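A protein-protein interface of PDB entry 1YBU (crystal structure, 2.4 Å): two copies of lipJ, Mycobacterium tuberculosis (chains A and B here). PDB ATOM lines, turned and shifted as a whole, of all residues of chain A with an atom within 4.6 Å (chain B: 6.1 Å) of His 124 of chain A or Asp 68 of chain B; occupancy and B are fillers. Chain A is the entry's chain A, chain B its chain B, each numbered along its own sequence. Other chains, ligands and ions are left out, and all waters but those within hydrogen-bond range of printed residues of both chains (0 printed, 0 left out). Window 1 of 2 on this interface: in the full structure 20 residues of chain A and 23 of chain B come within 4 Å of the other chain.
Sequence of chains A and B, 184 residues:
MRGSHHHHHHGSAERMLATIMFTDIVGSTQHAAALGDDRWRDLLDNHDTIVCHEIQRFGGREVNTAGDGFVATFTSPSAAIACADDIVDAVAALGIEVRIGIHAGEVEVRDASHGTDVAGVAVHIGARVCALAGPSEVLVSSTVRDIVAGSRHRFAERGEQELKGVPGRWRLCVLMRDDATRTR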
ATOM      1  N   GLY A 120     -17.129  -4.334  -8.388  1.00  0.00           N
ATOM      2  CA  GLY A 120     -18.193  -4.132  -7.436  1.00  0.00           C
ATOM      3  C   GLY A 120     -18.719  -2.752  -7.699  1.00  0.00           C
ATOM      4  O   GLY A 120     -18.099  -2.013  -8.451  1.00  0.00           O
ATOM      5  N   VAL A 121     -19.850  -2.392  -7.114  1.00  0.00           N
ATOM      6  CA  VAL A 121     -20.384  -1.052  -7.324  1.00  0.00           C
ATOM      7  C   VAL A 121     -19.420   0.009  -6.760  1.00  0.00           C
ATOM      8  O   VAL A 121     -19.510   1.189  -7.132  1.00  0.00           O
ATOM      9  CB  VAL A 121     -21.785  -0.921  -6.661  1.00  0.00           C
ATOM     10  CG1 VAL A 121     -21.800  -1.658  -5.352  1.00  0.00           C
ATOM     11  CG2 VAL A 121     -22.140   0.532  -6.400  1.00  0.00           C
ATOM     12  N   ALA A 122     -18.505  -0.383  -5.863  1.00  0.00           N
ATOM     13  CA  ALA A 122     -17.558   0.600  -5.312  1.00  0.00           C
ATOM     14  C   ALA A 122     -16.683   1.125  -6.456  1.00  0.00           C
ATOM     15  O   ALA A 122     -16.346   2.316  -6.505  1.00  0.00           O
ATOM     16  CB  ALA A 122     -16.657  -0.034  -4.211  1.00  0.00           C
ATOM     17  N   VAL A 123     -16.311   0.216  -7.359  1.00  0.00           N
ATOM     18  CA  VAL A 123     -15.492   0.559  -8.516  1.00  0.00           C
ATOM     19  C   VAL A 123     -16.237   1.563  -9.384  1.00  0.00           C
ATOM     20  O   VAL A 123     -15.675   2.574  -9.807  1.00  0.00           O
ATOM     21  CB  VAL A 123     -15.183  -0.677  -9.347  1.00  0.00           C
ATOM     22  CG1 VAL A 123     -14.377  -0.297 -10.565  1.00  0.00           C
ATOM     23  CG2 VAL A 123     -14.423  -1.680  -8.498  1.00  0.00           C
ATOM     24  N   HIS A 124     -17.515   1.307  -9.630  1.00  0.00           N
ATOM     25  CA  HIS A 124     -18.295   2.227 -10.441  1.00  0.00           C
ATOM     26  C   HIS A 124     -18.479   3.581  -9.797  1.00  0.00           C
ATOM     27  O   HIS A 124     -18.646   4.586 -10.489  1.00  0.00           O
ATOM     28  CB  HIS A 124     -19.668   1.634 -10.776  1.00  0.00           C
ATOM     29  CG  HIS A 124     -19.607   0.456 -11.701  1.00  0.00           C
ATOM     30  ND1 HIS A 124     -20.735  -0.222 -12.115  1.00  0.00           N
ATOM     31  CD2 HIS A 124     -18.556  -0.190 -12.260  1.00  0.00           C
ATOM     32  CE1 HIS A 124     -20.381  -1.239 -12.880  1.00  0.00           C
ATOM     33  NE2 HIS A 124     -19.063  -1.243 -12.982  1.00  0.00           N
ATOM     34  N   ILE A 125     -18.477   3.615  -8.472  1.00  0.00           N
ATOM     35  CA  ILE A 125     -18.647   4.885  -7.770  1.00  0.00           C
ATOM     36  C   ILE A 125     -17.355   5.687  -7.910  1.00  0.00           C
ATOM     37  O   ILE A 125     -17.402   6.876  -8.161  1.00  0.00           O
ATOM     38  CB  ILE A 125     -19.027   4.658  -6.266  1.00  0.00           C
ATOM     39  CG1 ILE A 125     -20.407   3.984  -6.207  1.00  0.00           C
ATOM     40  CG2 ILE A 125     -19.050   6.011  -5.500  1.00  0.00           C
ATOM     41  CD1 ILE A 125     -20.798   3.414  -4.853  1.00  0.00           C
ATOM     42  N   GLY A 126     -16.214   5.029  -7.754  1.00  0.00           N
ATOM     43  CA  GLY A 126     -14.952   5.720  -7.931  1.00  0.00           C
ATOM     44  C   GLY A 126     -14.870   6.358  -9.321  1.00  0.00           C
ATOM     45  O   GLY A 126     -14.754   7.588  -9.452  1.00  0.00           O
ATOM     46  N   ALA A 127     -14.976   5.520 -10.357  1.00  0.00           N
ATOM     47  CA  ALA A 127     -14.916   5.992 -11.733  1.00  0.00           C
ATOM     48  C   ALA A 127     -15.861   7.153 -11.894  1.00  0.00           C
ATOM     49  O   ALA A 127     -15.524   8.148 -12.530  1.00  0.00           O
ATOM     50  CB  ALA A 127     -15.293   4.867 -12.710  1.00  0.00           C
ATOM     51  N   ARG A 128     -17.037   7.062 -11.288  1.00  0.00           N
ATOM     52  CA  ARG A 128     -17.998   8.139 -11.431  1.00  0.00           C
ATOM     53  C   ARG A 128     -17.569   9.433 -10.748  1.00  0.00           C
ATOM     54  O   ARG A 128     -17.922  10.525 -11.198  1.00  0.00           O
ATOM     55  CB  ARG A 128     -19.368   7.703 -10.917  1.00  0.00           C
ATOM     56  CG  ARG A 128     -20.430   8.778 -11.062  1.00  0.00           C
ATOM     57  CD  ARG A 128     -21.151   8.808 -12.402  1.00  0.00           C
ATOM     58  NE  ARG A 128     -20.330   8.907 -13.603  1.00  0.00           N
ATOM     59  CZ  ARG A 128     -19.653   7.894 -14.133  1.00  0.00           C
ATOM     60  NH1 ARG A 128     -19.681   6.698 -13.571  1.00  0.00           N
ATOM     61  NH2 ARG A 128     -18.963   8.071 -15.243  1.00  0.00           N
ATOM     62  N   THR B  23     -15.998  -2.554 -26.947  1.00  0.00           N
ATOM     63  CA  THR B  23     -17.213  -3.170 -26.398  1.00  0.00           C
ATOM     64  C   THR B  23     -17.471  -2.677 -24.957  1.00  0.00           C
ATOM     65  O   THR B  23     -16.538  -2.332 -24.222  1.00  0.00           O
ATOM     66  CB  THR B  23     -17.113  -4.708 -26.383  1.00  0.00           C
ATOM     67  OG1 THR B  23     -16.196  -5.115 -25.372  1.00  0.00           O
ATOM     68  CG2 THR B  23     -16.631  -5.241 -27.719  1.00  0.00           C
ATOM     69  N   ASP B  24     -18.737  -2.623 -24.553  1.00  0.00           N
ATOM     70  CA  ASP B  24     -19.116  -2.187 -23.212  1.00  0.00           C
ATOM     71  C   ASP B  24     -20.478  -2.720 -22.818  1.00  0.00           C
ATOM     72  O   ASP B  24     -21.409  -2.712 -23.603  1.00  0.00           O
ATOM     73  CB  ASP B  24     -19.129  -0.661 -23.106  1.00  0.00           C
ATOM     74  CG  ASP B  24     -19.437  -0.167 -21.682  1.00  0.00           C
ATOM     75  OD1 ASP B  24     -20.534   0.404 -21.465  1.00  0.00           O
ATOM     76  OD2 ASP B  24     -18.579  -0.333 -20.775  1.00  0.00           O
ATOM     77  N   ILE B  25     -20.585  -3.155 -21.569  1.00  0.00           N
ATOM     78  CA  ILE B  25     -21.841  -3.699 -21.062  1.00  0.00           C
ATOM     79  C   ILE B  25     -22.841  -2.589 -20.806  1.00  0.00           C
ATOM     80  O   ILE B  25     -22.503  -1.579 -20.208  1.00  0.00           O
ATOM     81  CB  ILE B  25     -21.595  -4.484 -19.796  1.00  0.00           C
ATOM     82  CG1 ILE B  25     -20.646  -5.640 -20.100  1.00  0.00           C
ATOM     83  CG2 ILE B  25     -22.909  -5.002 -19.223  1.00  0.00           C
ATOM     84  CD1 ILE B  25     -20.373  -6.542 -18.922  1.00  0.00           C
ATOM     85  N   SER B  28     -24.265  -1.593 -16.755  1.00  0.00           N
ATOM     86  CA  SER B  28     -23.514  -2.475 -15.877  1.00  0.00           C
ATOM     87  C   SER B  28     -23.657  -2.020 -14.441  1.00  0.00           C
ATOM     88  O   SER B  28     -23.073  -2.604 -13.548  1.00  0.00           O
ATOM     89  CB  SER B  28     -22.028  -2.426 -16.213  1.00  0.00           C
ATOM     90  OG  SER B  28     -21.550  -1.079 -16.202  1.00  0.00           O
ATOM     91  N   THR B  29     -24.454  -1.008 -14.185  1.00  0.00           N
ATOM     92  CA  THR B  29     -24.477  -0.527 -12.836  1.00  0.00           C
ATOM     93  C   THR B  29     -25.787  -0.841 -12.182  1.00  0.00           C
ATOM     94  O   THR B  29     -25.927  -0.907 -10.950  1.00  0.00           O
ATOM     95  CB  THR B  29     -24.153   0.957 -12.874  1.00  0.00           C
ATOM     96  OG1 THR B  29     -22.828   1.135 -12.378  1.00  0.00           O
ATOM     97  CG2 THR B  29     -25.137   1.759 -12.112  1.00  0.00           C
ATOM     98  N   ALA B  32     -25.162  -4.678 -11.341  1.00  0.00           N
ATOM     99  CA  ALA B  32     -24.424  -4.990 -10.129  1.00  0.00           C
ATOM    100  C   ALA B  32     -25.332  -4.736  -8.918  1.00  0.00           C
ATOM    101  O   ALA B  32     -25.359  -5.536  -7.988  1.00  0.00           O
ATOM    102  CB  ALA B  32     -23.172  -4.117 -10.040  1.00  0.00           C
ATOM    103  N   TRP B  40     -22.385 -10.271  -9.574  1.00  0.00           N
ATOM    104  CA  TRP B  40     -21.894  -9.366 -10.604  1.00  0.00           C
ATOM    105  C   TRP B  40     -20.483  -9.757 -11.009  1.00  0.00           C
ATOM    106  O   TRP B  40     -20.140  -9.727 -12.189  1.00  0.00           O
ATOM    107  CB  TRP B  40     -21.908  -7.930 -10.104  1.00  0.00           C
ATOM    108  CG  TRP B  40     -21.200  -6.980 -11.009  1.00  0.00           C
ATOM    109  CD1 TRP B  40     -20.067  -6.271 -10.725  1.00  0.00           C
ATOM    110  CD2 TRP B  40     -21.581  -6.611 -12.339  1.00  0.00           C
ATOM    111  NE1 TRP B  40     -19.724  -5.480 -11.793  1.00  0.00           N
ATOM    112  CE2 TRP B  40     -20.635  -5.668 -12.798  1.00  0.00           C
ATOM    113  CE3 TRP B  40     -22.631  -6.984 -13.189  1.00  0.00           C
ATOM    114  CZ2 TRP B  40     -20.707  -5.091 -14.072  1.00  0.00           C
ATOM    115  CZ3 TRP B  40     -22.701  -6.410 -14.457  1.00  0.00           C
ATOM    116  CH2 TRP B  40     -21.743  -5.473 -14.884  1.00  0.00           C
ATOM    117  N   LEU B  44     -19.441 -11.018 -14.783  1.00  0.00           N
ATOM    118  CA  LEU B  44     -18.355 -10.234 -15.378  1.00  0.00           C
ATOM    119  C   LEU B  44     -17.276 -11.193 -15.873  1.00  0.00           C
ATOM    120  O   LEU B  44     -16.717 -10.995 -16.960  1.00  0.00           O
ATOM    121  CB  LEU B  44     -17.762  -9.253 -14.338  1.00  0.00           C
ATOM    122  CG  LEU B  44     -17.296  -7.859 -14.801  1.00  0.00           C
ATOM    123  CD1 LEU B  44     -18.414  -7.161 -15.568  1.00  0.00           C
ATOM    124  CD2 LEU B  44     -16.876  -7.011 -13.608  1.00  0.00           C
ATOM    125  N   HIS B  47     -18.675 -13.101 -19.029  1.00  0.00           N
ATOM    126  CA  HIS B  47     -18.631 -12.170 -20.148  1.00  0.00           C
ATOM    127  C   HIS B  47     -17.227 -12.072 -20.744  1.00  0.00           C
ATOM    128  O   HIS B  47     -17.037 -12.250 -21.949  1.00  0.00           O
ATOM    129  CB  HIS B  47     -19.118 -10.788 -19.666  1.00  0.00           C
ATOM    130  CG  HIS B  47     -18.744  -9.640 -20.560  1.00  0.00           C
ATOM    131  ND1 HIS B  47     -17.465  -9.141 -20.636  1.00  0.00           N
ATOM    132  CD2 HIS B  47     -19.504  -8.867 -21.372  1.00  0.00           C
ATOM    133  CE1 HIS B  47     -17.445  -8.110 -21.464  1.00  0.00           C
ATOM    134  NE2 HIS B  47     -18.670  -7.921 -21.924  1.00  0.00           N
ATOM    135  N   THR B  65      -8.468  -3.853 -21.652  1.00  0.00           N
ATOM    136  CA  THR B  65      -9.772  -3.390 -21.139  1.00  0.00           C
ATOM    137  C   THR B  65     -10.287  -1.957 -21.307  1.00  0.00           C
ATOM    138  O   THR B  65      -9.512  -0.990 -21.265  1.00  0.00           O
ATOM    139  CB  THR B  65     -10.004  -3.773 -19.650  1.00  0.00           C
ATOM    140  OG1 THR B  65      -9.928  -2.596 -18.836  1.00  0.00           O
ATOM    141  CG2 THR B  65      -8.977  -4.788 -19.197  1.00  0.00           C
ATOM    142  N   ALA B  66     -11.609  -1.864 -21.537  1.00  0.00           N
ATOM    143  CA  ALA B  66     -12.388  -0.624 -21.705  1.00  0.00           C
ATOM    144  C   ALA B  66     -13.319  -0.642 -20.489  1.00  0.00           C
ATOM    145  O   ALA B  66     -14.545  -0.386 -20.567  1.00  0.00           O
ATOM    146  CB  ALA B  66     -13.202  -0.699 -22.985  1.00  0.00           C
ATOM    147  N   GLY B  67     -12.653  -0.943 -19.373  1.00  0.00           N
ATOM    148  CA  GLY B  67     -13.242  -1.085 -18.057  1.00  0.00           C
ATOM    149  C   GLY B  67     -14.061  -2.350 -18.168  1.00  0.00           C
ATOM    150  O   GLY B  67     -13.541  -3.479 -18.248  1.00  0.00           O
ATOM    151  N   ASP B  68     -15.369  -2.118 -18.177  1.00  0.00           N
ATOM    152  CA  ASP B  68     -16.386  -3.157 -18.333  1.00  0.00           C
ATOM    153  C   ASP B  68     -16.449  -3.336 -19.835  1.00  0.00           C
ATOM    154  O   ASP B  68     -17.483  -3.095 -20.458  1.00  0.00           O
ATOM    155  CB  ASP B  68     -17.761  -2.667 -17.892  1.00  0.00           C
ATOM    156  CG  ASP B  68     -17.979  -2.777 -16.387  1.00  0.00           C
ATOM    157  OD1 ASP B  68     -18.528  -1.822 -15.796  1.00  0.00           O
ATOM    158  OD2 ASP B  68     -17.633  -3.817 -15.792  1.00  0.00           O
ATOM    159  N   GLY B  69     -15.347  -3.734 -20.436  1.00  0.00           N
ATOM    160  CA  GLY B  69     -15.416  -3.898 -21.861  1.00  0.00           C
ATOM    161  C   GLY B  69     -14.064  -4.148 -22.426  1.00  0.00           C
ATOM    162  O   GLY B  69     -13.066  -4.216 -21.714  1.00  0.00           O
ATOM    163  N   PHE B  70     -14.019  -4.280 -23.731  1.00  0.00           N
ATOM    164  CA  PHE B  70     -12.751  -4.545 -24.361  1.00  0.00           C
ATOM    165  C   PHE B  70     -12.434  -3.573 -25.468  1.00  0.00           C
ATOM    166  O   PHE B  70     -13.255  -2.764 -25.884  1.00  0.00           O
ATOM    167  CB  PHE B  70     -12.734  -5.962 -24.936  1.00  0.00           C
ATOM    168  CG  PHE B  70     -12.710  -7.042 -23.906  1.00  0.00           C
ATOM    169  CD1 PHE B  70     -13.832  -7.316 -23.131  1.00  0.00           C
ATOM    170  CD2 PHE B  70     -11.562  -7.805 -23.716  1.00  0.00           C
ATOM    171  CE1 PHE B  70     -13.809  -8.326 -22.188  1.00  0.00           C
ATOM    172  CE2 PHE B  70     -11.536  -8.824 -22.763  1.00  0.00           C
ATOM    173  CZ  PHE B  70     -12.662  -9.082 -22.001  1.00  0.00           C
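Among the printed residues, pairs that only touch across the chains: His 124 of chain A with Ser 28 of chain B (3.1 Å).
OG1 of Thr 29 of chain B sits at hydrogen-bond distance from ND1 of His 124 of chain A, at 2.5 Å. A ring nitrogen (NE2) of His 124 of chain A lies within hydrogen-bond range of the side-chain carboxylate (OD1) of Asp 68 of chain B, at 2.9 Å.
Of the 15 printed residues of chain B, 3 touch a printed residue of chain A. Printed residues of chain B that touch a printed residue of chain A: Ser 28, Thr 29 and Asp 68.
No position is printed for both chains.
Of chain B, only Ser 28, Thr 29 and Asp 68 come within 4 Å of His 124 of chain A. Asp 68 of chain B touches one residue of chain A. Of the printed residues of chain A, Thr 29 of chain B touches His 124 (2.5 Å). Of the printed residues of chain A, Ser 28 of chain B touches His 124. Asp 24 of chain B touches none of the printed residues of chain A.
The backbone NH (N) of Ile 25 of chain B sits at hydrogen-bond distance from the backbone carbonyl oxygen (O) of Asp 68 of chain B. The side-chain hydroxyl (OG) of Ser 28 of chain B is in hydrogen-bond range of the side-chain carboxylate (OD1) of Asp 68 of chain B, at 3.1 Å.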
